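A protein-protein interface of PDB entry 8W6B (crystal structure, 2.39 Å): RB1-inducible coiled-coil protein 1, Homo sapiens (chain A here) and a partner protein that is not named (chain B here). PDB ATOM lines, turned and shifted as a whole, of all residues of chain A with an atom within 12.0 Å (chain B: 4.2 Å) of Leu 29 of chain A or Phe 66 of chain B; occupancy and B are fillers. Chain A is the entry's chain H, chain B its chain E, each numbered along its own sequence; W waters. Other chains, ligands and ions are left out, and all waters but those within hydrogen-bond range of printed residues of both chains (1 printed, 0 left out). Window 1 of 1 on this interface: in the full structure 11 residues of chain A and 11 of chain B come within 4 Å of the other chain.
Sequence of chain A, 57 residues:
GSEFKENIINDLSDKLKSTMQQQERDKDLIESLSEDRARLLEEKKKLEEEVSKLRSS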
ATOM      1  N   MET A  20      -4.518  21.100 -27.969  1.00  0.00           N
ATOM      2  CA  MET A  20      -4.447  22.271 -27.108  1.00  0.00           C
ATOM      3  C   MET A  20      -4.680  21.890 -25.656  1.00  0.00           C
ATOM      4  O   MET A  20      -3.977  22.373 -24.763  1.00  0.00           O
ATOM      5  CB  MET A  20      -5.426  23.335 -27.581  1.00  0.00           C
ATOM      6  CG  MET A  20      -4.857  24.083 -28.779  1.00  0.00           C
ATOM      7  SD  MET A  20      -6.029  25.060 -29.722  1.00  0.00           S
ATOM      8  CE  MET A  20      -6.573  26.192 -28.444  1.00  0.00           C
ATOM      9  N   GLN A  21      -5.618  20.973 -25.404  1.00  0.00           N
ATOM     10  CA  GLN A  21      -5.855  20.508 -24.039  1.00  0.00           C
ATOM     11  C   GLN A  21      -4.639  19.773 -23.496  1.00  0.00           C
ATOM     12  O   GLN A  21      -4.273  19.939 -22.328  1.00  0.00           O
ATOM     13  CB  GLN A  21      -7.099  19.615 -23.981  1.00  0.00           C
ATOM     14  CG  GLN A  21      -8.402  20.387 -24.105  1.00  0.00           C
ATOM     15  CD  GLN A  21      -9.653  19.495 -24.151  1.00  0.00           C
ATOM     16  OE1 GLN A  21      -9.737  18.550 -24.947  1.00  0.00           O
ATOM     17  NE2 GLN A  21     -10.642  19.817 -23.310  1.00  0.00           N
ATOM     18  N   GLN A  22      -3.997  18.957 -24.330  1.00  0.00           N
ATOM     19  CA  GLN A  22      -2.719  18.390 -23.928  1.00  0.00           C
ATOM     20  C   GLN A  22      -1.718  19.495 -23.600  1.00  0.00           C
ATOM     21  O   GLN A  22      -1.005  19.419 -22.590  1.00  0.00           O
ATOM     22  CB  GLN A  22      -2.173  17.483 -25.027  1.00  0.00           C
ATOM     23  CG  GLN A  22      -0.923  16.743 -24.600  1.00  0.00           C
ATOM     24  CD  GLN A  22      -1.142  15.918 -23.329  1.00  0.00           C
ATOM     25  OE1 GLN A  22      -2.167  15.253 -23.173  1.00  0.00           O
ATOM     26  NE2 GLN A  22      -0.179  15.977 -22.410  1.00  0.00           N
ATOM     27  N   GLN A  23      -1.689  20.553 -24.416  1.00  0.00           N
ATOM     28  CA  GLN A  23      -0.668  21.579 -24.251  1.00  0.00           C
ATOM     29  C   GLN A  23      -0.821  22.313 -22.928  1.00  0.00           C
ATOM     30  O   GLN A  23       0.170  22.769 -22.355  1.00  0.00           O
ATOM     31  CB  GLN A  23      -0.721  22.565 -25.413  1.00  0.00           C
ATOM     32  CG  GLN A  23       0.242  23.727 -25.293  1.00  0.00           C
ATOM     33  CD  GLN A  23       0.622  24.281 -26.655  1.00  0.00           C
ATOM     34  OE1 GLN A  23       1.238  23.588 -27.478  1.00  0.00           O
ATOM     35  NE2 GLN A  23       0.230  25.527 -26.912  1.00  0.00           N
ATOM     36  N   GLU A  24      -2.049  22.432 -22.428  1.00  0.00           N
ATOM     37  CA  GLU A  24      -2.233  23.066 -21.133  1.00  0.00           C
ATOM     38  C   GLU A  24      -1.703  22.183 -20.008  1.00  0.00           C
ATOM     39  O   GLU A  24      -1.118  22.696 -19.039  1.00  0.00           O
ATOM     40  CB  GLU A  24      -3.707  23.414 -20.927  1.00  0.00           C
ATOM     41  CG  GLU A  24      -3.978  24.902 -20.960  1.00  0.00           C
ATOM     42  CD  GLU A  24      -3.403  25.621 -19.747  1.00  0.00           C
ATOM     43  OE1 GLU A  24      -2.237  26.071 -19.817  1.00  0.00           O
ATOM     44  OE2 GLU A  24      -4.114  25.747 -18.726  1.00  0.00           O
ATOM     45  N   ARG A  25      -1.875  20.861 -20.133  1.00  0.00           N
ATOM     46  CA  ARG A  25      -1.264  19.947 -19.175  1.00  0.00           C
ATOM     47  C   ARG A  25       0.254  20.058 -19.218  1.00  0.00           C
ATOM     48  O   ARG A  25       0.917  20.089 -18.180  1.00  0.00           O
ATOM     49  CB  ARG A  25      -1.710  18.511 -19.460  1.00  0.00           C
ATOM     50  CG  ARG A  25      -3.184  18.251 -19.111  1.00  0.00           C
ATOM     51  CD  ARG A  25      -3.988  17.480 -20.170  1.00  0.00           C
ATOM     52  NE  ARG A  25      -5.335  17.257 -19.659  1.00  0.00           N
ATOM     53  CZ  ARG A  25      -5.822  16.081 -19.282  1.00  0.00           C
ATOM     54  NH1 ARG A  25      -5.078  14.985 -19.390  1.00  0.00           N
ATOM     55  NH2 ARG A  25      -7.057  16.007 -18.795  1.00  0.00           N
ATOM     56  N   ASP A  26       0.814  20.140 -20.421  1.00  0.00           N
ATOM     57  CA  ASP A  26       2.256  20.207 -20.586  1.00  0.00           C
ATOM     58  C   ASP A  26       2.825  21.459 -19.947  1.00  0.00           C
ATOM     59  O   ASP A  26       3.839  21.396 -19.249  1.00  0.00           O
ATOM     60  CB  ASP A  26       2.598  20.156 -22.075  1.00  0.00           C
ATOM     61  CG  ASP A  26       2.371  18.780 -22.668  1.00  0.00           C
ATOM     62  OD1 ASP A  26       2.026  17.850 -21.901  1.00  0.00           O
ATOM     63  OD2 ASP A  26       2.557  18.629 -23.893  1.00  0.00           O
ATOM     64  N   LYS A  27       2.176  22.601 -20.169  1.00  0.00           N
ATOM     65  CA  LYS A  27       2.630  23.855 -19.582  1.00  0.00           C
ATOM     66  C   LYS A  27       2.663  23.768 -18.052  1.00  0.00           C
ATOM     67  O   LYS A  27       3.671  24.120 -17.425  1.00  0.00           O
ATOM     68  CB  LYS A  27       1.737  24.999 -20.068  1.00  0.00           C
ATOM     69  CG  LYS A  27       1.651  26.159 -19.119  1.00  0.00           C
ATOM     70  CD  LYS A  27       0.708  27.244 -19.607  1.00  0.00           C
ATOM     71  CE  LYS A  27       0.860  28.495 -18.755  1.00  0.00           C
ATOM     72  NZ  LYS A  27       0.063  29.609 -19.310  1.00  0.00           N
ATOM     73  N   ASP A  28       1.595  23.238 -17.439  1.00  0.00           N
ATOM     74  CA  ASP A  28       1.570  23.080 -15.984  1.00  0.00           C
ATOM     75  C   ASP A  28       2.689  22.161 -15.492  1.00  0.00           C
ATOM     76  O   ASP A  28       3.336  22.447 -14.474  1.00  0.00           O
ATOM     77  CB  ASP A  28       0.201  22.552 -15.536  1.00  0.00           C
ATOM     78  CG  ASP A  28      -0.911  23.597 -15.696  1.00  0.00           C
ATOM     79  OD1 ASP A  28      -0.613  24.776 -16.032  1.00  0.00           O
ATOM     80  OD2 ASP A  28      -2.088  23.223 -15.514  1.00  0.00           O
ATOM     81  N   LEU A  29       2.957  21.067 -16.216  1.00  0.00           N
ATOM     82  CA  LEU A  29       4.021  20.154 -15.800  1.00  0.00           C
ATOM     83  C   LEU A  29       5.401  20.779 -15.972  1.00  0.00           C
ATOM     84  O   LEU A  29       6.301  20.556 -15.153  1.00  0.00           O
ATOM     85  CB  LEU A  29       3.932  18.848 -16.586  1.00  0.00           C
ATOM     86  CG  LEU A  29       4.963  17.808 -16.187  1.00  0.00           C
ATOM     87  CD1 LEU A  29       4.630  17.273 -14.784  1.00  0.00           C
ATOM     88  CD2 LEU A  29       5.014  16.713 -17.230  1.00  0.00           C
ATOM     89  N   ILE A  30       5.590  21.559 -17.030  1.00  0.00           N
ATOM     90  CA  ILE A  30       6.889  22.181 -17.251  1.00  0.00           C
ATOM     91  C   ILE A  30       7.169  23.222 -16.177  1.00  0.00           C
ATOM     92  O   ILE A  30       8.280  23.280 -15.629  1.00  0.00           O
ATOM     93  CB  ILE A  30       6.968  22.764 -18.671  1.00  0.00           C
ATOM     94  CG1 ILE A  30       7.185  21.603 -19.648  1.00  0.00           C
ATOM     95  CG2 ILE A  30       8.122  23.735 -18.776  1.00  0.00           C
ATOM     96  CD1 ILE A  30       6.936  21.913 -21.080  1.00  0.00           C
ATOM     97  N   GLU A  31       6.159  24.028 -15.835  1.00  0.00           N
ATOM     98  CA  GLU A  31       6.280  24.983 -14.735  1.00  0.00           C
ATOM     99  C   GLU A  31       6.721  24.314 -13.426  1.00  0.00           C
ATOM    100  O   GLU A  31       7.694  24.750 -12.794  1.00  0.00           O
ATOM    101  CB  GLU A  31       4.959  25.754 -14.566  1.00  0.00           C
ATOM    102  CG  GLU A  31       5.064  27.160 -15.175  1.00  0.00           C
ATOM    103  CD  GLU A  31       3.737  27.765 -15.558  1.00  0.00           C
ATOM    104  OE1 GLU A  31       2.708  27.370 -14.977  1.00  0.00           O
ATOM    105  OE2 GLU A  31       3.726  28.647 -16.444  1.00  0.00           O
ATOM    106  N   SER A  32       6.049  23.232 -13.013  1.00  0.00           N
ATOM    107  CA  SER A  32       6.436  22.608 -11.746  1.00  0.00           C
ATOM    108  C   SER A  32       7.805  21.959 -11.864  1.00  0.00           C
ATOM    109  O   SER A  32       8.675  22.170 -11.012  1.00  0.00           O
ATOM    110  CB  SER A  32       5.410  21.572 -11.290  1.00  0.00           C
ATOM    111  OG  SER A  32       4.126  22.062 -11.548  1.00  0.00           O
ATOM    112  N   LEU A  33       8.019  21.179 -12.926  1.00  0.00           N
ATOM    113  CA  LEU A  33       9.282  20.465 -13.061  1.00  0.00           C
ATOM    114  C   LEU A  33      10.454  21.433 -13.122  1.00  0.00           C
ATOM    115  O   LEU A  33      11.480  21.203 -12.473  1.00  0.00           O
ATOM    116  CB  LEU A  33       9.284  19.559 -14.308  1.00  0.00           C
ATOM    117  CG  LEU A  33       8.450  18.278 -14.421  1.00  0.00           C
ATOM    118  CD1 LEU A  33       8.562  17.692 -15.830  1.00  0.00           C
ATOM    119  CD2 LEU A  33       8.857  17.241 -13.390  1.00  0.00           C
ATOM    120  N   SER A  34      10.333  22.519 -13.899  1.00  0.00           N
ATOM    121  CA  SER A  34      11.495  23.381 -14.058  1.00  0.00           C
ATOM    122  C   SER A  34      11.807  24.095 -12.746  1.00  0.00           C
ATOM    123  O   SER A  34      12.971  24.154 -12.335  1.00  0.00           O
ATOM    124  CB  SER A  34      11.304  24.375 -15.217  1.00  0.00           C
ATOM    125  OG  SER A  34      10.210  25.240 -15.015  1.00  0.00           O
ATOM    126  N   GLU A  35      10.775  24.563 -12.035  1.00  0.00           N
ATOM    127  CA  GLU A  35      10.994  25.147 -10.705  1.00  0.00           C
ATOM    128  C   GLU A  35      11.595  24.131  -9.736  1.00  0.00           C
ATOM    129  O   GLU A  35      12.546  24.442  -9.009  1.00  0.00           O
ATOM    130  CB  GLU A  35       9.687  25.711 -10.132  1.00  0.00           C
ATOM    131  CG  GLU A  35       9.442  27.180 -10.434  1.00  0.00           C
ATOM    132  CD  GLU A  35       7.964  27.587 -10.372  1.00  0.00           C
ATOM    133  OE1 GLU A  35       7.368  27.818 -11.454  1.00  0.00           O
ATOM    134  OE2 GLU A  35       7.411  27.706  -9.255  1.00  0.00           O
ATOM    135  N   ASP A  36      11.079  22.904  -9.729  1.00  0.00           N
ATOM    136  CA  ASP A  36      11.528  21.964  -8.711  1.00  0.00           C
ATOM    137  C   ASP A  36      12.945  21.484  -8.990  1.00  0.00           C
ATOM    138  O   ASP A  36      13.732  21.292  -8.056  1.00  0.00           O
ATOM    139  CB  ASP A  36      10.579  20.767  -8.596  1.00  0.00           C
ATOM    140  CG  ASP A  36      10.812  19.998  -7.326  1.00  0.00           C
ATOM    141  OD1 ASP A  36      10.829  18.744  -7.340  1.00  0.00           O
ATOM    142  OD2 ASP A  36      11.000  20.676  -6.290  1.00  0.00           O
ATOM    143  N   ARG A  37      13.282  21.269 -10.267  1.00  0.00           N
ATOM    144  CA  ARG A  37      14.638  20.853 -10.603  1.00  0.00           C
ATOM    145  C   ARG A  37      15.629  21.904 -10.149  1.00  0.00           C
ATOM    146  O   ARG A  37      16.683  21.573  -9.592  1.00  0.00           O
ATOM    147  CB  ARG A  37      14.779  20.592 -12.113  1.00  0.00           C
ATOM    148  CG  ARG A  37      15.956  19.707 -12.491  1.00  0.00           C
ATOM    149  CD  ARG A  37      16.017  19.421 -13.987  1.00  0.00           C
ATOM    150  NE  ARG A  37      16.574  20.586 -14.667  1.00  0.00           N
ATOM    151  CZ  ARG A  37      17.770  20.615 -15.238  1.00  0.00           C
ATOM    152  NH1 ARG A  37      18.550  19.540 -15.263  1.00  0.00           N
ATOM    153  NH2 ARG A  37      18.176  21.725 -15.811  1.00  0.00           N
ATOM    154  N   ALA A  38      15.287  23.181 -10.350  1.00  0.00           N
ATOM    155  CA  ALA A  38      16.171  24.262  -9.940  1.00  0.00           C
ATOM    156  C   ALA A  38      16.426  24.191  -8.450  1.00  0.00           C
ATOM    157  O   ALA A  38      17.577  24.226  -8.008  1.00  0.00           O
ATOM    158  CB  ALA A  38      15.575  25.615 -10.329  1.00  0.00           C
ATOM    159  N   LEU A  40      16.012  21.538  -6.416  1.00  0.00           N
ATOM    160  CA  LEU A  40      16.850  20.357  -6.195  1.00  0.00           C
ATOM    161  C   LEU A  40      18.329  20.640  -6.490  1.00  0.00           C
ATOM    162  O   LEU A  40      19.209  20.214  -5.730  1.00  0.00           O
ATOM    163  CB  LEU A  40      16.356  19.176  -7.040  1.00  0.00           C
ATOM    164  CG  LEU A  40      15.130  18.360  -6.570  1.00  0.00           C
ATOM    165  CD1 LEU A  40      14.633  17.340  -7.615  1.00  0.00           C
ATOM    166  CD2 LEU A  40      15.386  17.663  -5.234  1.00  0.00           C
ATOM    167  N   TRP B  49      -4.320  16.329  -7.460  1.00  0.00           N
ATOM    168  CA  TRP B  49      -3.624  15.832  -8.631  1.00  0.00           C
ATOM    169  C   TRP B  49      -3.232  14.379  -8.423  1.00  0.00           C
ATOM    170  O   TRP B  49      -3.186  13.868  -7.299  1.00  0.00           O
ATOM    171  CB  TRP B  49      -2.401  16.703  -8.954  1.00  0.00           C
ATOM    172  CG  TRP B  49      -1.512  16.983  -7.792  1.00  0.00           C
ATOM    173  CD1 TRP B  49      -1.710  17.910  -6.823  1.00  0.00           C
ATOM    174  CD2 TRP B  49      -0.262  16.344  -7.486  1.00  0.00           C
ATOM    175  NE1 TRP B  49      -0.662  17.892  -5.923  1.00  0.00           N
ATOM    176  CE2 TRP B  49       0.242  16.946  -6.318  1.00  0.00           C
ATOM    177  CE3 TRP B  49       0.476  15.335  -8.085  1.00  0.00           C
ATOM    178  CZ2 TRP B  49       1.440  16.559  -5.738  1.00  0.00           C
ATOM    179  CZ3 TRP B  49       1.675  14.976  -7.520  1.00  0.00           C
ATOM    180  CH2 TRP B  49       2.149  15.583  -6.369  1.00  0.00           C
ATOM    181  N   VAL B  50      -2.991  13.714  -9.543  1.00  0.00           N
ATOM    182  CA  VAL B  50      -2.513  12.339  -9.584  1.00  0.00           C
ATOM    183  C   VAL B  50      -1.085  12.357 -10.128  1.00  0.00           C
ATOM    184  O   VAL B  50      -0.817  12.926 -11.201  1.00  0.00           O
ATOM    185  CB  VAL B  50      -3.454  11.438 -10.417  1.00  0.00           C
ATOM    186  CG1 VAL B  50      -2.857  10.027 -10.635  1.00  0.00           C
ATOM    187  CG2 VAL B  50      -4.811  11.297  -9.727  1.00  0.00           C
ATOM    188  N   GLY B  51      -0.173  11.766  -9.373  1.00  0.00           N
ATOM    189  CA  GLY B  51       1.204  11.651  -9.803  1.00  0.00           C
ATOM    190  C   GLY B  51       1.664  10.213  -9.985  1.00  0.00           C
ATOM    191  O   GLY B  51       1.098   9.288  -9.400  1.00  0.00           O
ATOM    192  N   TYR B  63       7.257  13.127  -6.786  1.00  0.00           N
ATOM    193  CA  TYR B  63       6.594  12.652  -7.990  1.00  0.00           C
ATOM    194  C   TYR B  63       7.561  12.587  -9.188  1.00  0.00           C
ATOM    195  O   TYR B  63       8.584  13.283  -9.259  1.00  0.00           O
ATOM    196  CB  TYR B  63       5.400  13.552  -8.327  1.00  0.00           C
ATOM    197  CG  TYR B  63       5.804  14.942  -8.776  1.00  0.00           C
ATOM    198  CD1 TYR B  63       6.000  15.967  -7.853  1.00  0.00           C
ATOM    199  CD2 TYR B  63       5.984  15.230 -10.125  1.00  0.00           C
ATOM    200  CE1 TYR B  63       6.374  17.254  -8.277  1.00  0.00           C
ATOM    201  CE2 TYR B  63       6.350  16.486 -10.545  1.00  0.00           C
ATOM    202  CZ  TYR B  63       6.563  17.498  -9.627  1.00  0.00           C
ATOM    203  OH  TYR B  63       6.945  18.755 -10.079  1.00  0.00           O
ATOM    204  N   THR B  65       6.006  12.616 -12.629  1.00  0.00           N
ATOM    205  CA  THR B  65       5.203  13.581 -13.359  1.00  0.00           C
ATOM    206  C   THR B  65       3.811  13.508 -12.759  1.00  0.00           C
ATOM    207  O   THR B  65       3.500  12.610 -11.970  1.00  0.00           O
ATOM    208  CB  THR B  65       5.114  13.271 -14.865  1.00  0.00           C
ATOM    209  OG1 THR B  65       4.536  11.969 -15.051  1.00  0.00           O
ATOM    210  CG2 THR B  65       6.460  13.318 -15.544  1.00  0.00           C
ATOM    211  N   PHE B  66       2.948  14.416 -13.183  1.00  0.00           N
ATOM    212  CA  PHE B  66       1.643  14.507 -12.543  1.00  0.00           C
ATOM    213  C   PHE B  66       0.666  15.164 -13.503  1.00  0.00           C
ATOM    214  O   PHE B  66       1.058  15.802 -14.481  1.00  0.00           O
ATOM    215  CB  PHE B  66       1.715  15.316 -11.240  1.00  0.00           C
ATOM    216  CG  PHE B  66       1.691  16.785 -11.470  1.00  0.00           C
ATOM    217  CD1 PHE B  66       2.882  17.474 -11.659  1.00  0.00           C
ATOM    218  CD2 PHE B  66       0.484  17.476 -11.575  1.00  0.00           C
ATOM    219  CE1 PHE B  66       2.882  18.833 -11.909  1.00  0.00           C
ATOM    220  CE2 PHE B  66       0.469  18.810 -11.838  1.00  0.00           C
ATOM    221  CZ  PHE B  66       1.687  19.504 -12.014  1.00  0.00           C
ATOM    222  N   LEU B  67      -0.612  15.023 -13.189  1.00  0.00           N
ATOM    223  CA  LEU B  67      -1.657  15.749 -13.887  1.00  0.00           C
ATOM    224  C   LEU B  67      -2.645  16.233 -12.843  1.00  0.00           C
ATOM    225  O   LEU B  67      -2.924  15.512 -11.880  1.00  0.00           O
ATOM    226  CB  LEU B  67      -2.373  14.865 -14.901  1.00  0.00           C
ATOM    227  CG  LEU B  67      -1.718  14.475 -16.233  1.00  0.00           C
ATOM    228  CD1 LEU B  67      -2.524  13.309 -16.884  1.00  0.00           C
ATOM    229  CD2 LEU B  67      -1.663  15.656 -17.185  1.00  0.00           C
ATOM    230  N   TRP B  68      -3.164  17.449 -13.020  1.00  0.00           N
ATOM    231  CA  TRP B  68      -4.257  17.888 -12.159  1.00  0.00           C
ATOM    232  C   TRP B  68      -5.419  16.916 -12.298  1.00  0.00           C
ATOM    233  O   TRP B  68      -5.743  16.477 -13.405  1.00  0.00           O
ATOM    234  CB  TRP B  68      -4.699  19.304 -12.515  1.00  0.00           C
ATOM    235  CG  TRP B  68      -3.601  20.297 -12.323  1.00  0.00           C
ATOM    236  CD1 TRP B  68      -2.943  21.004 -13.296  1.00  0.00           C
ATOM    237  CD2 TRP B  68      -3.004  20.671 -11.085  1.00  0.00           C
ATOM    238  NE1 TRP B  68      -1.985  21.800 -12.733  1.00  0.00           N
ATOM    239  CE2 TRP B  68      -1.991  21.614 -11.378  1.00  0.00           C
ATOM    240  CE3 TRP B  68      -3.240  20.318  -9.749  1.00  0.00           C
ATOM    241  CZ2 TRP B  68      -1.205  22.203 -10.389  1.00  0.00           C
ATOM    242  CZ3 TRP B  68      -2.456  20.909  -8.754  1.00  0.00           C
ATOM    243  CH2 TRP B  68      -1.449  21.844  -9.086  1.00  0.00           C
ATOM    244  N   TYR B  91       5.001  11.394 -20.482  1.00  0.00           N
ATOM    245  CA  TYR B  91       4.969  11.613 -19.042  1.00  0.00           C
ATOM    246  C   TYR B  91       5.576  10.447 -18.276  1.00  0.00           C
ATOM    247  O   TYR B  91       5.662  10.501 -17.040  1.00  0.00           O
ATOM    248  CB  TYR B  91       3.525  11.823 -18.541  1.00  0.00           C
ATOM    249  CG  TYR B  91       2.942  13.209 -18.753  1.00  0.00           C
ATOM    250  CD1 TYR B  91       3.061  13.852 -19.973  1.00  0.00           C
ATOM    251  CD2 TYR B  91       2.243  13.865 -17.730  1.00  0.00           C
ATOM    252  CE1 TYR B  91       2.513  15.107 -20.183  1.00  0.00           C
ATOM    253  CE2 TYR B  91       1.695  15.142 -17.936  1.00  0.00           C
ATOM    254  CZ  TYR B  91       1.826  15.749 -19.175  1.00  0.00           C
ATOM    255  OH  TYR B  91       1.297  17.010 -19.432  1.00  0.00           O
HETATM  256  O   HOH W   1       0.154  18.260 -15.857  1.00  0.00           O
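Water W1 lies within hydrogen-bond range of O of Phe 66 of chain B (3.0 Å) and O of Arg 25 of chain A (3.1 Å).
NE1 of Trp 68 of chain B is in hydrogen-bond range of OD2 of Asp 28 of chain A (3.1 Å).
The side-chain hydroxyl (OH) of Tyr 91 of chain B lies within hydrogen-bond range of the side-chain amide nitrogen (NE2) of Gln 22 of chain A, at 3.5 Å.
The side-chain hydroxyl of Tyr 91 of chain B lies close to the backbone carbonyl oxygen of Arg 25 of chain A, at 3.3 Å.
OH of Tyr 91 of chain B is in hydrogen-bond range of OD1 of Asp 26 of chain A (2.7 Å).
Printed residues of chain B that touch a printed residue of chain A: Tyr 63, Thr 65, Phe 66, Leu 67, Trp 68 and Tyr 91.
Hydrophobic or aromatic side chains of chain B within 4 Å of the printed part of chain A: Tyr 63, Phe 66, Leu 67, Trp 68 and Tyr 91.
Printed residues of chain A that touch a printed residue of chain B: Gln 22, Arg 25, Asp 26, Asp 28, Leu 29, Ser 32 and Leu 33.
Hydrophobic or aromatic side chains of chain A within 4 Å of the printed part of chain B: Leu 29 and Leu 33.
The backbone NH (N) of Leu 67 of chain B is in hydrogen-bond range of the backbone carbonyl oxygen (O) of Val 50 of chain B, at 2.9 Å.
The side-chain hydroxyl of Thr 65 of chain B sits at hydrogen-bond distance from the backbone carbonyl oxygen of Tyr 91 of chain B, 2.7 Å away.
The side-chain carboxylate (OD1) of Asp 26 of chain A sits at hydrogen-bond distance from the side-chain amide nitrogen (NE2) of Gln 22 of chain A.
The side-chain hydroxyl (OG) of Ser 32 of chain A is in hydrogen-bond range of the backbone carbonyl oxygen (O) of Asp 28 of chain A (3.1 Å).
CG of Arg 25 of chain A touches CD2 of Leu 67 of chain B, 3.6 Å away.
Leu 29 of chain A touches Thr 65 of chain B (CD1 to CA, 3.999 Å).
Leu 29 of chain A touches Phe 66 of chain B.
Leu 29 of chain A touches Tyr 91 of chain B.
Ser 32 of chain A touches Tyr 63 of chain B.
CE1 of Phe 66 of chain B touches OG of Ser 32 of chain A (3.5 Å).
Tyr 63 of chain B touches Leu 33 of chain A (CE2 to CD2, 3.9 Å).
Printed residues of chain B within 4 Å of Leu 29 of chain A: Thr 65, Phe 66 and Tyr 91.
Phe 66 of chain B touches just these residues of chain A: Leu 29 (3.6 Å) and Ser 32 (3.5 Å).
No residue of chain A comes within 4 Å of Trp 49 of chain B.
No residue of chain A comes within 4 Å of Gly 51 of chain B.
Of chain A, only Ser 32 (3.4 Å) and Leu 33 (3.9 Å) come within 4 Å of Tyr 63 of chain B.
Printed residues of chain A within 4 Å of Leu 67 of chain B: Arg 25.
Of chain A, only Asp 28 comes within 4 Å of Trp 68 of chain B.
Printed residues of chain B within 4 Å of Asp 28 of chain A: Trp 68.
Printed residues of chain B within 4 Å of Asp 26 of chain A: Tyr 91.
Of the printed residues of chain B, Gln 22 of chain A touches Tyr 91.
Met 20 of chain A touches none of the printed residues of chain B.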
